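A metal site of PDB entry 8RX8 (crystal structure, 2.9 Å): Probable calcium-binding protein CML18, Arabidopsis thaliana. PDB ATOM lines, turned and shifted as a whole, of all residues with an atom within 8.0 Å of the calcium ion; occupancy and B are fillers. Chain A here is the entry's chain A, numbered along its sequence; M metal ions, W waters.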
ATOM      1  N   TYR A 109      -5.210 -14.739   0.517  1.00  0.00           N
ATOM      2  CA  TYR A 109      -5.280 -15.256  -0.848  1.00  0.00           C
ATOM      3  C   TYR A 109      -4.420 -16.501  -0.972  1.00  0.00           C
ATOM      4  O   TYR A 109      -3.313 -16.569  -0.428  1.00  0.00           O
ATOM      5  CB  TYR A 109      -4.805 -14.206  -1.863  1.00  0.00           C
ATOM      6  CG  TYR A 109      -5.672 -12.959  -1.924  1.00  0.00           C
ATOM      7  CD1 TYR A 109      -5.478 -11.916  -1.030  1.00  0.00           C
ATOM      8  CD2 TYR A 109      -6.678 -12.844  -2.876  1.00  0.00           C
ATOM      9  CE1 TYR A 109      -6.260 -10.781  -1.086  1.00  0.00           C
ATOM     10  CE2 TYR A 109      -7.476 -11.713  -2.930  1.00  0.00           C
ATOM     11  CZ  TYR A 109      -7.262 -10.679  -2.039  1.00  0.00           C
ATOM     12  OH  TYR A 109      -8.047  -9.552  -2.091  1.00  0.00           O
ATOM     13  N   ILE A 110      -4.945 -17.493  -1.689  1.00  0.00           N
ATOM     14  CA  ILE A 110      -4.215 -18.719  -1.992  1.00  0.00           C
ATOM     15  C   ILE A 110      -3.585 -18.552  -3.372  1.00  0.00           C
ATOM     16  O   ILE A 110      -4.277 -18.610  -4.390  1.00  0.00           O
ATOM     17  CB  ILE A 110      -5.133 -19.944  -1.951  1.00  0.00           C
ATOM     18  CG1 ILE A 110      -5.694 -20.141  -0.546  1.00  0.00           C
ATOM     19  CG2 ILE A 110      -4.376 -21.195  -2.386  1.00  0.00           C
ATOM     20  CD1 ILE A 110      -6.640 -21.322  -0.448  1.00  0.00           C
ATOM     21  N   ILE A 135      -7.282 -23.662 -10.574  1.00  0.00           N
ATOM     22  CA  ILE A 135      -7.446 -22.226 -10.442  1.00  0.00           C
ATOM     23  C   ILE A 135      -8.539 -21.721 -11.391  1.00  0.00           C
ATOM     24  O   ILE A 135      -9.467 -21.031 -10.963  1.00  0.00           O
ATOM     25  CB  ILE A 135      -6.117 -21.505 -10.691  1.00  0.00           C
ATOM     26  CG1 ILE A 135      -5.111 -21.820  -9.573  1.00  0.00           C
ATOM     27  CG2 ILE A 135      -6.325 -19.997 -10.782  1.00  0.00           C
ATOM     28  CD1 ILE A 135      -5.539 -21.324  -8.217  1.00  0.00           C
ATOM     29  N   ALA A 138     -11.846 -22.758  -9.740  1.00  0.00           N
ATOM     30  CA  ALA A 138     -12.215 -22.177  -8.459  1.00  0.00           C
ATOM     31  C   ALA A 138     -12.092 -20.659  -8.414  1.00  0.00           C
ATOM     32  O   ALA A 138     -12.723 -20.022  -7.567  1.00  0.00           O
ATOM     33  CB  ALA A 138     -11.361 -22.770  -7.333  1.00  0.00           C
ATOM     34  N   ASP A 139     -11.299 -20.066  -9.303  1.00  0.00           N
ATOM     35  CA  ASP A 139     -11.124 -18.614  -9.319  1.00  0.00           C
ATOM     36  C   ASP A 139     -12.236 -17.957 -10.124  1.00  0.00           C
ATOM     37  O   ASP A 139     -12.498 -18.340 -11.275  1.00  0.00           O
ATOM     38  CB  ASP A 139      -9.757 -18.250  -9.902  1.00  0.00           C
ATOM     39  CG  ASP A 139      -9.688 -16.814 -10.378  1.00  0.00           C
ATOM     40  OD1 ASP A 139      -9.693 -15.901  -9.525  1.00  0.00           O
ATOM     41  OD2 ASP A 139      -9.621 -16.604 -11.606  1.00  0.00           O
ATOM     42  N   ARG A 140     -12.893 -16.968  -9.521  1.00  0.00           N
ATOM     43  CA  ARG A 140     -14.036 -16.284 -10.102  1.00  0.00           C
ATOM     44  C   ARG A 140     -13.744 -14.833 -10.422  1.00  0.00           C
ATOM     45  O   ARG A 140     -14.053 -14.371 -11.529  1.00  0.00           O
ATOM     46  CB  ARG A 140     -15.252 -16.392  -9.160  1.00  0.00           C
ATOM     47  CG  ARG A 140     -16.145 -17.588  -9.442  1.00  0.00           C
ATOM     48  CD  ARG A 140     -16.560 -18.298  -8.155  1.00  0.00           C
ATOM     49  NE  ARG A 140     -17.843 -17.832  -7.641  1.00  0.00           N
ATOM     50  CZ  ARG A 140     -17.986 -16.968  -6.641  1.00  0.00           C
ATOM     51  NH1 ARG A 140     -16.950 -16.437  -6.032  1.00  0.00           N
ATOM     52  NH2 ARG A 140     -19.208 -16.631  -6.254  1.00  0.00           N
ATOM     53  N   ASP A 141     -13.159 -14.082  -9.495  1.00  0.00           N
ATOM     54  CA  ASP A 141     -12.834 -12.679  -9.724  1.00  0.00           C
ATOM     55  C   ASP A 141     -11.604 -12.481 -10.594  1.00  0.00           C
ATOM     56  O   ASP A 141     -11.254 -11.334 -10.901  1.00  0.00           O
ATOM     57  CB  ASP A 141     -12.664 -11.940  -8.388  1.00  0.00           C
ATOM     58  CG  ASP A 141     -11.363 -12.311  -7.684  1.00  0.00           C
ATOM     59  OD1 ASP A 141     -11.041 -13.517  -7.637  1.00  0.00           O
ATOM     60  OD2 ASP A 141     -10.691 -11.398  -7.175  1.00  0.00           O
ATOM     61  N   GLY A 142     -10.941 -13.562 -11.007  1.00  0.00           N
ATOM     62  CA  GLY A 142      -9.916 -13.486 -12.027  1.00  0.00           C
ATOM     63  C   GLY A 142      -8.572 -12.943 -11.606  1.00  0.00           C
ATOM     64  O   GLY A 142      -7.744 -12.653 -12.477  1.00  0.00           O
ATOM     65  N   ASP A 143      -8.309 -12.794 -10.315  1.00  0.00           N
ATOM     66  CA  ASP A 143      -7.030 -12.232  -9.883  1.00  0.00           C
ATOM     67  C   ASP A 143      -5.885 -13.217  -9.952  1.00  0.00           C
ATOM     68  O   ASP A 143      -4.725 -12.820  -9.785  1.00  0.00           O
ATOM     69  CB  ASP A 143      -7.148 -11.655  -8.466  1.00  0.00           C
ATOM     70  CG  ASP A 143      -7.616 -12.682  -7.445  1.00  0.00           C
ATOM     71  OD1 ASP A 143      -7.609 -13.893  -7.749  1.00  0.00           O
ATOM     72  OD2 ASP A 143      -8.005 -12.269  -6.327  1.00  0.00           O
ATOM     73  N   GLY A 144      -6.160 -14.505 -10.186  1.00  0.00           N
ATOM     74  CA  GLY A 144      -5.153 -15.535 -10.248  1.00  0.00           C
ATOM     75  C   GLY A 144      -5.010 -16.338  -8.979  1.00  0.00           C
ATOM     76  O   GLY A 144      -4.568 -17.490  -9.028  1.00  0.00           O
ATOM     77  N   CYS A 145      -5.365 -15.757  -7.835  1.00  0.00           N
ATOM     78  CA  CYS A 145      -5.334 -16.456  -6.562  1.00  0.00           C
ATOM     79  C   CYS A 145      -6.754 -16.868  -6.163  1.00  0.00           C
ATOM     80  O   CYS A 145      -7.690 -16.820  -6.975  1.00  0.00           O
ATOM     81  CB  CYS A 145      -4.673 -15.571  -5.499  1.00  0.00           C
ATOM     82  SG  CYS A 145      -4.125 -13.953  -6.104  1.00  0.00           S
ATOM     83  N   ILE A 146      -6.924 -17.270  -4.919  1.00  0.00           N
ATOM     84  CA  ILE A 146      -8.214 -17.751  -4.413  1.00  0.00           C
ATOM     85  C   ILE A 146      -8.401 -17.167  -3.020  1.00  0.00           C
ATOM     86  O   ILE A 146      -7.598 -17.425  -2.118  1.00  0.00           O
ATOM     87  CB  ILE A 146      -8.275 -19.289  -4.353  1.00  0.00           C
ATOM     88  CG1 ILE A 146      -8.333 -19.876  -5.773  1.00  0.00           C
ATOM     89  CG2 ILE A 146      -9.472 -19.745  -3.529  1.00  0.00           C
ATOM     90  CD1 ILE A 146      -8.341 -21.374  -5.794  1.00  0.00           C
ATOM     91  N   ASP A 147      -9.465 -16.382  -2.848  1.00  0.00           N
ATOM     92  CA  ASP A 147      -9.796 -15.870  -1.529  1.00  0.00           C
ATOM     93  C   ASP A 147     -10.730 -16.847  -0.809  1.00  0.00           C
ATOM     94  O   ASP A 147     -11.052 -17.924  -1.323  1.00  0.00           O
ATOM     95  CB  ASP A 147     -10.417 -14.472  -1.624  1.00  0.00           C
ATOM     96  CG  ASP A 147     -11.681 -14.450  -2.459  1.00  0.00           C
ATOM     97  OD1 ASP A 147     -12.720 -14.935  -1.970  1.00  0.00           O
ATOM     98  OD2 ASP A 147     -11.642 -13.906  -3.587  1.00  0.00           O
ATOM     99  N   PHE A 148     -11.181 -16.460   0.384  1.00  0.00           N
ATOM    100  CA  PHE A 148     -11.982 -17.363   1.199  1.00  0.00           C
ATOM    101  C   PHE A 148     -13.369 -17.591   0.600  1.00  0.00           C
ATOM    102  O   PHE A 148     -13.917 -18.694   0.690  1.00  0.00           O
ATOM    103  CB  PHE A 148     -12.091 -16.822   2.623  1.00  0.00           C
ATOM    104  CG  PHE A 148     -12.878 -17.699   3.551  1.00  0.00           C
ATOM    105  CD1 PHE A 148     -12.459 -18.992   3.833  1.00  0.00           C
ATOM    106  CD2 PHE A 148     -14.044 -17.237   4.152  1.00  0.00           C
ATOM    107  CE1 PHE A 148     -13.177 -19.803   4.678  1.00  0.00           C
ATOM    108  CE2 PHE A 148     -14.761 -18.047   4.997  1.00  0.00           C
ATOM    109  CZ  PHE A 148     -14.332 -19.337   5.270  1.00  0.00           C
ATOM    110  N   GLU A 150     -14.271 -17.534  -2.715  1.00  0.00           N
ATOM    111  CA  GLU A 150     -14.114 -18.501  -3.794  1.00  0.00           C
ATOM    112  C   GLU A 150     -13.738 -19.872  -3.247  1.00  0.00           C
ATOM    113  O   GLU A 150     -14.126 -20.892  -3.829  1.00  0.00           O
ATOM    114  CB  GLU A 150     -13.058 -18.030  -4.789  1.00  0.00           C
ATOM    115  CG  GLU A 150     -13.046 -16.531  -5.036  1.00  0.00           C
ATOM    116  CD  GLU A 150     -11.906 -16.116  -5.940  1.00  0.00           C
ATOM    117  OE1 GLU A 150     -10.801 -15.828  -5.419  1.00  0.00           O
ATOM    118  OE2 GLU A 150     -12.098 -16.078  -7.172  1.00  0.00           O
ATOM    119  N   PHE A 151     -12.988 -19.907  -2.142  1.00  0.00           N
ATOM    120  CA  PHE A 151     -12.625 -21.175  -1.515  1.00  0.00           C
ATOM    121  C   PHE A 151     -13.865 -21.936  -1.067  1.00  0.00           C
ATOM    122  O   PHE A 151     -14.022 -23.139  -1.373  1.00  0.00           O
ATOM    123  CB  PHE A 151     -11.693 -20.904  -0.343  1.00  0.00           C
ATOM    124  CG  PHE A 151     -11.249 -22.128   0.395  1.00  0.00           C
ATOM    125  CD1 PHE A 151     -10.274 -22.960  -0.148  1.00  0.00           C
ATOM    126  CD2 PHE A 151     -11.799 -22.453   1.623  1.00  0.00           C
ATOM    127  CE1 PHE A 151      -9.864 -24.089   0.533  1.00  0.00           C
ATOM    128  CE2 PHE A 151     -11.389 -23.582   2.304  1.00  0.00           C
ATOM    129  CZ  PHE A 151     -10.424 -24.401   1.755  1.00  0.00           C
HETATM  130 CA    CA M   1      -9.524 -15.260  -7.323  1.00  0.00          CA
HETATM  131  O   HOH W   1      -9.782 -13.454  -5.084  1.00  0.00           O
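OD1 of Asp 139 is bound to the calcium ion, 2.3 Å away. OD1 of Asp 141 binds the calcium ion. OE1 of Glu 150 binds the calcium ion (2.4 Å). The calcium ion is bound by OD1 of Asp 143. O of Cys 145 is bound to the calcium ion, 2.4 Å away. The calcium ion is bound by the side-chain carboxylate (OE2) of Glu 150 (2.7 Å). Water W1 binds the calcium ion (2.9 Å).
Within 4 Å of the calcium ion: Asp 139, Asp 141, Asp 143, Cys 145 and Glu 150.
The side-chain carboxylate (OD2) of Asp 139 lies close to the backbone NH (N) of Gly 142 (3.4 Å). N of Glu 150 is in hydrogen-bond range of OD1 of Asp 147 (3.1 Å). The backbone NH (N) of Arg 140 sits close to the side-chain carboxylate (OE2) of Glu 150.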
